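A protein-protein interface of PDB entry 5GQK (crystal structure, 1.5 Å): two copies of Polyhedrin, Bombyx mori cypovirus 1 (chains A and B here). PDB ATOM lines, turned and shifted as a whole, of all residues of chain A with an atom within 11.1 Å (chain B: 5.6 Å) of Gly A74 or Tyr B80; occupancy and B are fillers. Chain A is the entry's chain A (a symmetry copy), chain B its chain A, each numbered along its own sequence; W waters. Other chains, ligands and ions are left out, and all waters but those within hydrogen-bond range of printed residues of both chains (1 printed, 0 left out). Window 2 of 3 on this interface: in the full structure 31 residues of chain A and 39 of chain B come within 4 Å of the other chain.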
ATOM      1  N   GLU A  70     -22.262   4.492  15.695  1.00  0.00           N
ATOM      2  CA  GLU A  70     -21.213   3.502  15.594  1.00  0.00           C
ATOM      3  C   GLU A  70     -21.149   2.557  16.770  1.00  0.00           C
ATOM      4  O   GLU A  70     -21.071   3.018  17.924  1.00  0.00           O
ATOM      5  CB  GLU A  70     -19.846   4.193  15.460  1.00  0.00           C
ATOM      6  CG  GLU A  70     -18.692   3.186  15.192  1.00  0.00           C
ATOM      7  CD  GLU A  70     -17.362   3.855  14.947  1.00  0.00           C
ATOM      8  OE1 GLU A  70     -17.279   5.075  15.105  1.00  0.00           O
ATOM      9  OE2 GLU A  70     -16.378   3.166  14.557  1.00  0.00           O
ATOM     10  N   TYR A  71     -21.018   1.243  16.460  1.00  0.00           N
ATOM     11  CA  TYR A  71     -20.806   0.209  17.492  1.00  0.00           C
ATOM     12  C   TYR A  71     -19.669  -0.672  16.987  1.00  0.00           C
ATOM     13  O   TYR A  71     -19.742  -1.205  15.891  1.00  0.00           O
ATOM     14  CB  TYR A  71     -22.091  -0.610  17.703  1.00  0.00           C
ATOM     15  CG  TYR A  71     -21.884  -1.593  18.804  1.00  0.00           C
ATOM     16  CD1 TYR A  71     -21.863  -1.165  20.151  1.00  0.00           C
ATOM     17  CD2 TYR A  71     -21.636  -2.937  18.501  1.00  0.00           C
ATOM     18  CE1 TYR A  71     -21.629  -2.101  21.185  1.00  0.00           C
ATOM     19  CE2 TYR A  71     -21.376  -3.877  19.504  1.00  0.00           C
ATOM     20  CZ  TYR A  71     -21.359  -3.460  20.819  1.00  0.00           C
ATOM     21  OH  TYR A  71     -21.126  -4.419  21.808  1.00  0.00           O
ATOM     22  N   ARG A  72     -18.607  -0.764  17.762  1.00  0.00           N
ATOM     23  CA  ARG A  72     -17.427  -1.499  17.361  1.00  0.00           C
ATOM     24  C   ARG A  72     -17.495  -2.819  18.108  1.00  0.00           C
ATOM     25  O   ARG A  72     -17.306  -2.849  19.301  1.00  0.00           O
ATOM     26  CB  ARG A  72     -16.159  -0.727  17.757  1.00  0.00           C
ATOM     27  CG  ARG A  72     -16.079   0.694  17.157  1.00  0.00           C
ATOM     28  CD  ARG A  72     -14.676   1.245  17.321  1.00  0.00           C
ATOM     29  NE  ARG A  72     -14.317   1.364  18.719  1.00  0.00           N
ATOM     30  CZ  ARG A  72     -13.084   1.586  19.149  1.00  0.00           C
ATOM     31  NH1 ARG A  72     -12.086   1.725  18.263  1.00  0.00           N
ATOM     32  NH2 ARG A  72     -12.834   1.667  20.450  1.00  0.00           N
ATOM     33  N   GLU A  73     -17.805  -3.897  17.388  1.00  0.00           N
ATOM     34  CA  GLU A  73     -17.943  -5.238  18.027  1.00  0.00           C
ATOM     35  C   GLU A  73     -16.656  -5.683  18.681  1.00  0.00           C
ATOM     36  O   GLU A  73     -15.555  -5.641  18.031  1.00  0.00           O
ATOM     37  CB  GLU A  73     -18.378  -6.284  16.988  1.00  0.00           C
ATOM     38  CG  GLU A  73     -19.783  -6.100  16.438  1.00  0.00           C
ATOM     39  CD  GLU A  73     -20.061  -7.090  15.310  1.00  0.00           C
ATOM     40  OE1 GLU A  73     -19.569  -8.249  15.361  1.00  0.00           O
ATOM     41  OE2 GLU A  73     -20.741  -6.710  14.357  1.00  0.00           O
ATOM     42  N   GLY A  74     -16.767  -6.128  19.916  1.00  0.00           N
ATOM     43  CA  GLY A  74     -15.611  -6.653  20.637  1.00  0.00           C
ATOM     44  C   GLY A  74     -14.567  -5.609  21.056  1.00  0.00           C
ATOM     45  O   GLY A  74     -13.529  -5.969  21.561  1.00  0.00           O
ATOM     46  N   GLN A  75     -14.830  -4.315  20.853  1.00  0.00           N
ATOM     47  CA  GLN A  75     -13.985  -3.247  21.373  1.00  0.00           C
ATOM     48  C   GLN A  75     -14.745  -2.350  22.343  1.00  0.00           C
ATOM     49  O   GLN A  75     -15.973  -2.510  22.520  1.00  0.00           O
ATOM     50  CB  GLN A  75     -13.440  -2.444  20.173  1.00  0.00           C
ATOM     51  CG  GLN A  75     -12.331  -3.157  19.369  1.00  0.00           C
ATOM     52  CD  GLN A  75     -11.904  -2.307  18.170  1.00  0.00           C
ATOM     53  OE1 GLN A  75     -12.604  -2.257  17.182  1.00  0.00           O
ATOM     54  NE2 GLN A  75     -10.790  -1.594  18.286  1.00  0.00           N
ATOM     55  N   HIS A  76     -14.023  -1.463  23.024  1.00  0.00           N
ATOM     56  CA  HIS A  76     -14.630  -0.445  23.891  1.00  0.00           C
ATOM     57  C   HIS A  76     -15.450   0.541  23.114  1.00  0.00           C
ATOM     58  O   HIS A  76     -15.040   1.003  22.042  1.00  0.00           O
ATOM     59  CB  HIS A  76     -13.578   0.270  24.744  1.00  0.00           C
ATOM     60  CG  HIS A  76     -13.109  -0.563  25.898  1.00  0.00           C
ATOM     61  ND1 HIS A  76     -13.976  -1.082  26.842  1.00  0.00           N
ATOM     62  CD2 HIS A  76     -11.873  -1.009  26.240  1.00  0.00           C
ATOM     63  CE1 HIS A  76     -13.293  -1.789  27.729  1.00  0.00           C
ATOM     64  NE2 HIS A  76     -12.013  -1.756  27.388  1.00  0.00           N
ATOM     65  N   ASN A  77     -16.608   0.889  23.696  1.00  0.00           N
ATOM     66  CA  ASN A  77     -17.530   1.804  23.040  1.00  0.00           C
ATOM     67  C   ASN A  77     -17.992   2.971  23.939  1.00  0.00           C
ATOM     68  O   ASN A  77     -18.992   3.619  23.591  1.00  0.00           O
ATOM     69  CB  ASN A  77     -18.738   1.050  22.552  1.00  0.00           C
ATOM     70  CG  ASN A  77     -18.433   0.178  21.332  1.00  0.00           C
ATOM     71  OD1 ASN A  77     -18.273   0.702  20.188  1.00  0.00           O
ATOM     72  ND2 ASN A  77     -18.397  -1.151  21.542  1.00  0.00           N
ATOM     73  N   ASP A  78     -17.280   3.250  25.038  1.00  0.00           N
ATOM     74  CA  ASP A  78     -17.649   4.328  25.982  1.00  0.00           C
ATOM     75  C   ASP A  78     -19.162   4.104  26.332  1.00  0.00           C
ATOM     76  O   ASP A  78     -19.935   5.096  26.311  1.00  0.00           O
ATOM     77  CB  ASP A  78     -17.553   5.749  25.366  1.00  0.00           C
ATOM     78  CG  ASP A  78     -16.237   6.462  25.615  1.00  0.00           C
ATOM     79  OD1 ASP A  78     -15.328   5.853  26.186  1.00  0.00           O
ATOM     80  OD2 ASP A  78     -16.116   7.679  25.235  1.00  0.00           O
ATOM     81  N   SER A  79     -19.566   2.843  26.561  1.00  0.00           N
ATOM     82  CA  SER A  79     -21.016   2.547  26.660  1.00  0.00           C
ATOM     83  C   SER A  79     -21.814   3.422  27.608  1.00  0.00           C
ATOM     84  O   SER A  79     -22.928   3.862  27.237  1.00  0.00           O
ATOM     85  CB  SER A  79     -21.284   1.073  26.980  1.00  0.00           C
ATOM     86  OG  SER A  79     -21.123   0.365  25.769  1.00  0.00           O
ATOM     87  N   ASN A 209     -23.581  -4.566   8.827  1.00  0.00           N
ATOM     88  CA  ASN A 209     -22.157  -4.755   9.176  1.00  0.00           C
ATOM     89  C   ASN A 209     -21.461  -3.437   9.197  1.00  0.00           C
ATOM     90  O   ASN A 209     -21.864  -2.520   8.449  1.00  0.00           O
ATOM     91  CB  ASN A 209     -21.454  -5.667   8.158  1.00  0.00           C
ATOM     92  CG  ASN A 209     -20.053  -6.099   8.637  1.00  0.00           C
ATOM     93  OD1 ASN A 209     -19.867  -6.646   9.754  1.00  0.00           O
ATOM     94  ND2 ASN A 209     -19.044  -5.874   7.768  1.00  0.00           N
ATOM     95  N   ARG A 210     -20.432  -3.307  10.032  1.00  0.00           N
ATOM     96  CA  ARG A 210     -19.619  -2.072  10.026  1.00  0.00           C
ATOM     97  C   ARG A 210     -18.330  -2.449   9.310  1.00  0.00           C
ATOM     98  O   ARG A 210     -17.552  -3.252   9.830  1.00  0.00           O
ATOM     99  CB  ARG A 210     -19.290  -1.570  11.442  1.00  0.00           C
ATOM    100  CG  ARG A 210     -18.554  -0.225  11.406  1.00  0.00           C
ATOM    101  CD  ARG A 210     -18.297   0.293  12.811  1.00  0.00           C
ATOM    102  NE  ARG A 210     -17.376  -0.582  13.507  1.00  0.00           N
ATOM    103  CZ  ARG A 210     -16.047  -0.415  13.525  1.00  0.00           C
ATOM    104  NH1 ARG A 210     -15.461   0.691  12.995  1.00  0.00           N
ATOM    105  NH2 ARG A 210     -15.288  -1.340  14.156  1.00  0.00           N
ATOM    106  N   TYR A 211     -18.065  -1.813   8.204  1.00  0.00           N
ATOM    107  CA  TYR A 211     -16.751  -1.911   7.465  1.00  0.00           C
ATOM    108  C   TYR A 211     -15.816  -0.769   7.896  1.00  0.00           C
ATOM    109  O   TYR A 211     -16.254   0.289   8.317  1.00  0.00           O
ATOM    110  CB  TYR A 211     -17.013  -1.859   5.948  1.00  0.00           C
ATOM    111  CG  TYR A 211     -17.685  -3.159   5.441  1.00  0.00           C
ATOM    112  CD1 TYR A 211     -16.906  -4.306   5.177  1.00  0.00           C
ATOM    113  CD2 TYR A 211     -19.080  -3.247   5.311  1.00  0.00           C
ATOM    114  CE1 TYR A 211     -17.536  -5.481   4.755  1.00  0.00           C
ATOM    115  CE2 TYR A 211     -19.679  -4.403   4.850  1.00  0.00           C
ATOM    116  CZ  TYR A 211     -18.898  -5.513   4.584  1.00  0.00           C
ATOM    117  OH  TYR A 211     -19.574  -6.693   4.182  1.00  0.00           O
ATOM    118  N   TRP A 212     -14.518  -0.999   7.810  1.00  0.00           N
ATOM    119  CA  TRP A 212     -13.608  -0.046   8.387  1.00  0.00           C
ATOM    120  C   TRP A 212     -13.326   1.157   7.511  1.00  0.00           C
ATOM    121  O   TRP A 212     -12.797   2.105   8.009  1.00  0.00           O
ATOM    122  CB  TRP A 212     -12.280  -0.717   8.744  1.00  0.00           C
ATOM    123  CG  TRP A 212     -12.381  -1.657   9.876  1.00  0.00           C
ATOM    124  CD1 TRP A 212     -13.434  -1.815  10.769  1.00  0.00           C
ATOM    125  CD2 TRP A 212     -11.354  -2.562  10.259  1.00  0.00           C
ATOM    126  NE1 TRP A 212     -13.080  -2.795  11.718  1.00  0.00           N
ATOM    127  CE2 TRP A 212     -11.799  -3.228  11.445  1.00  0.00           C
ATOM    128  CE3 TRP A 212     -10.028  -2.803   9.776  1.00  0.00           C
ATOM    129  CZ2 TRP A 212     -10.997  -4.218  12.108  1.00  0.00           C
ATOM    130  CZ3 TRP A 212      -9.225  -3.801  10.444  1.00  0.00           C
ATOM    131  CH2 TRP A 212      -9.732  -4.498  11.590  1.00  0.00           C
ATOM    132  N   GLU A 216     -12.762  -0.459   1.782  1.00  0.00           N
ATOM    133  CA  GLU A 216     -13.164  -1.833   2.137  1.00  0.00           C
ATOM    134  C   GLU A 216     -14.575  -2.129   1.780  1.00  0.00           C
ATOM    135  O   GLU A 216     -14.889  -3.251   1.332  1.00  0.00           O
ATOM    136  CB  GLU A 216     -12.981  -2.046   3.625  1.00  0.00           C
ATOM    137  CG  GLU A 216     -13.212  -3.481   4.084  1.00  0.00           C
ATOM    138  CD  GLU A 216     -12.964  -3.554   5.557  1.00  0.00           C
ATOM    139  OE1 GLU A 216     -13.862  -3.242   6.361  1.00  0.00           O
ATOM    140  OE2 GLU A 216     -11.801  -3.869   5.895  1.00  0.00           O
ATOM    141  N   ASP B  78     -15.841 -14.647  22.498  1.00  0.00           N
ATOM    142  CA  ASP B  78     -14.751 -14.354  21.542  1.00  0.00           C
ATOM    143  C   ASP B  78     -15.256 -13.163  20.654  1.00  0.00           C
ATOM    144  O   ASP B  78     -15.105 -13.238  19.407  1.00  0.00           O
ATOM    145  CB  ASP B  78     -14.454 -15.525  20.566  1.00  0.00           C
ATOM    146  CG  ASP B  78     -13.340 -16.454  21.010  1.00  0.00           C
ATOM    147  OD1 ASP B  78     -12.828 -16.283  22.120  1.00  0.00           O
ATOM    148  OD2 ASP B  78     -12.958 -17.381  20.212  1.00  0.00           O
ATOM    149  N   SER B  79     -15.895 -12.155  21.272  1.00  0.00           N
ATOM    150  CA  SER B  79     -16.596 -11.129  20.463  1.00  0.00           C
ATOM    151  C   SER B  79     -15.790 -10.492  19.348  1.00  0.00           C
ATOM    152  O   SER B  79     -16.327 -10.332  18.225  1.00  0.00           O
ATOM    153  CB  SER B  79     -17.215 -10.031  21.334  1.00  0.00           C
ATOM    154  OG  SER B  79     -18.409 -10.568  21.865  1.00  0.00           O
ATOM    155  N   TYR B  80     -14.547 -10.120  19.653  1.00  0.00           N
ATOM    156  CA  TYR B  80     -13.716  -9.418  18.658  1.00  0.00           C
ATOM    157  C   TYR B  80     -13.333 -10.406  17.527  1.00  0.00           C
ATOM    158  O   TYR B  80     -13.492 -10.124  16.314  1.00  0.00           O
ATOM    159  CB  TYR B  80     -12.461  -8.715  19.248  1.00  0.00           C
ATOM    160  CG  TYR B  80     -11.835  -8.056  18.068  1.00  0.00           C
ATOM    161  CD1 TYR B  80     -12.393  -6.837  17.542  1.00  0.00           C
ATOM    162  CD2 TYR B  80     -10.761  -8.649  17.386  1.00  0.00           C
ATOM    163  CE1 TYR B  80     -11.871  -6.257  16.382  1.00  0.00           C
ATOM    164  CE2 TYR B  80     -10.258  -8.061  16.206  1.00  0.00           C
ATOM    165  CZ  TYR B  80     -10.821  -6.889  15.729  1.00  0.00           C
ATOM    166  OH  TYR B  80     -10.327  -6.301  14.567  1.00  0.00           O
ATOM    167  N   ASP B  81     -12.838 -11.578  17.912  1.00  0.00           N
ATOM    168  CA  ASP B  81     -12.460 -12.585  16.898  1.00  0.00           C
ATOM    169  C   ASP B  81     -13.647 -12.981  16.034  1.00  0.00           C
ATOM    170  O   ASP B  81     -13.477 -13.292  14.850  1.00  0.00           O
ATOM    171  CB  ASP B  81     -11.846 -13.842  17.561  1.00  0.00           C
ATOM    172  CG  ASP B  81     -11.006 -14.652  16.595  1.00  0.00           C
ATOM    173  OD1 ASP B  81     -10.145 -14.059  15.914  1.00  0.00           O
ATOM    174  OD2 ASP B  81     -11.188 -15.882  16.516  1.00  0.00           O
ATOM    175  N   GLU B  82     -14.842 -12.975  16.642  1.00  0.00           N
ATOM    176  CA  GLU B  82     -16.058 -13.366  15.896  1.00  0.00           C
ATOM    177  C   GLU B  82     -16.527 -12.272  14.904  1.00  0.00           C
ATOM    178  O   GLU B  82     -17.108 -12.618  13.876  1.00  0.00           O
ATOM    179  CB  GLU B  82     -17.181 -13.765  16.845  1.00  0.00           C
ATOM    180  CG  GLU B  82     -16.899 -15.113  17.532  1.00  0.00           C
ATOM    181  CD  GLU B  82     -16.833 -16.305  16.545  1.00  0.00           C
ATOM    182  OE1 GLU B  82     -17.588 -16.286  15.589  1.00  0.00           O
ATOM    183  OE2 GLU B  82     -16.071 -17.324  16.753  1.00  0.00           O
ATOM    184  N   TYR B  83     -16.249 -10.995  15.219  1.00  0.00           N
ATOM    185  CA  TYR B  83     -16.398  -9.900  14.224  1.00  0.00           C
ATOM    186  C   TYR B  83     -15.457 -10.259  13.028  1.00  0.00           C
ATOM    187  O   TYR B  83     -15.848 -10.162  11.836  1.00  0.00           O
ATOM    188  CB  TYR B  83     -16.006  -8.499  14.829  1.00  0.00           C
ATOM    189  CG  TYR B  83     -15.896  -7.445  13.748  1.00  0.00           C
ATOM    190  CD1 TYR B  83     -17.030  -6.810  13.219  1.00  0.00           C
ATOM    191  CD2 TYR B  83     -14.638  -7.133  13.199  1.00  0.00           C
ATOM    192  CE1 TYR B  83     -16.914  -5.881  12.155  1.00  0.00           C
ATOM    193  CE2 TYR B  83     -14.508  -6.210  12.162  1.00  0.00           C
ATOM    194  CZ  TYR B  83     -15.625  -5.571  11.684  1.00  0.00           C
ATOM    195  OH  TYR B  83     -15.427  -4.661  10.676  1.00  0.00           O
ATOM    196  N   GLU B  84     -14.200 -10.625  13.310  1.00  0.00           N
ATOM    197  CA  GLU B  84     -13.247 -10.927  12.209  1.00  0.00           C
ATOM    198  C   GLU B  84     -13.681 -12.187  11.413  1.00  0.00           C
ATOM    199  O   GLU B  84     -13.550 -12.230  10.188  1.00  0.00           O
ATOM    200  CB  GLU B  84     -11.833 -11.147  12.791  1.00  0.00           C
ATOM    201  CG  GLU B  84     -11.197  -9.857  13.333  1.00  0.00           C
ATOM    202  CD  GLU B  84     -10.863  -8.866  12.215  1.00  0.00           C
ATOM    203  OE1 GLU B  84     -10.846  -9.276  11.037  1.00  0.00           O
ATOM    204  OE2 GLU B  84     -10.674  -7.669  12.516  1.00  0.00           O
ATOM    205  N   VAL B  85     -14.260 -13.174  12.108  1.00  0.00           N
ATOM    206  CA  VAL B  85     -14.745 -14.393  11.428  1.00  0.00           C
ATOM    207  C   VAL B  85     -15.841 -13.938  10.455  1.00  0.00           C
ATOM    208  O   VAL B  85     -15.861 -14.354   9.287  1.00  0.00           O
ATOM    209  CB  VAL B  85     -15.388 -15.375  12.452  1.00  0.00           C
ATOM    210  CG1 VAL B  85     -16.330 -16.355  11.763  1.00  0.00           C
ATOM    211  CG2 VAL B  85     -14.343 -16.148  13.273  1.00  0.00           C
HETATM  212  O   HOH W   1     -19.046 -10.334  16.984  1.00  0.00           O
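The side-chain hydroxyl (OH) of Tyr B83 lies within hydrogen-bond range of the backbone carbonyl oxygen (O) of Arg A210. The indole nitrogen (NE1) of Trp A212 is in hydrogen-bond range of the side-chain hydroxyl (OH) of Tyr B83 (3.2 Å).
The side-chain hydroxyl (OH) of Tyr B80 is in hydrogen-bond range of the side-chain carboxylate (OE2) of Glu B84, at 2.5 Å. The side-chain carboxylate of Glu A70 is in salt-bridge range of the guanidinium group of Arg A210. O of Tyr A71 lies within hydrogen-bond range of NE of Arg A210 (3.4 Å). N of Trp A212 is in hydrogen-bond range of OE1 of Glu A216 (2.7 Å).
O of Glu A73 touches CD1 of Tyr B80 (3.4 Å). Tyr B83 touches Glu A73 (CB to OE1, 3.6 Å). Gly A74 touches Ser B79. O of Gly A74 touches CB of Tyr B80 (3.7 Å). Asn A209 touches Tyr B83. Trp A212 touches Tyr B80. Trp A212 touches Glu B84 (CH2 to OE2, 3.4 Å).
Of chain B, only Ser B79 and Tyr B80 come within 4 Å of Gly A74. Ser B79 touches one residue of chain A. No residue of chain A comes within 4 Å of Asp B81. Printed residues of chain A within 4 Å of Tyr B83: Glu A73, Asn A209, Arg A210 and Trp A212. Glu B84 touches just one residue of chain A: Trp A212. Of the printed residues of chain B, Arg A210 touches Tyr B83 (2.7 Å). Of the printed residues of chain B, Glu A73 touches Tyr B80 (3.4 Å) and Tyr B83 (3.6 Å). Printed residues of chain B within 4 Å of Trp A212: Tyr B80, Tyr B83 and Glu B84. The nearest printed residue of chain B that does not touch Gly A74 is Tyr B83 (5.7 Å). The nearest residue of chain A that does not touch Tyr B80 is Gln A75 (4.1 Å). The nearest printed residue of chain B that does not touch Glu A73 is Ser B79 (4.7 Å).
Of the 8 printed residues of chain B, 4 touch a printed residue of chain A. Printed residues of chain B that touch a printed residue of chain A: Ser B79, Tyr B80, Tyr B83 and Glu B84. Hydrophobic or aromatic side chains of chain B within 4 Å of the printed part of chain A: Tyr B80 and Tyr B83. Of the 15 printed residues of chain A, 5 touch a printed residue of chain B. Among the printed residues, no Asp or Glu carboxylate lies within 4 Å of a Lys or Arg side-chain nitrogen of the other chain.
Positions printed for both chains: 78 and 79. Of the 9 pairs that touch across the chains among the printed residues, none has its exchanged pair printed and touching as well.
Water W1 lies within hydrogen-bond range of the side-chain carboxylate (OE1) of Glu A73 (2.7 Å), the backbone carbonyl oxygen (O) of Ser B79 (3.0 Å) and the backbone NH (N) of Tyr B83 (3.4 Å).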
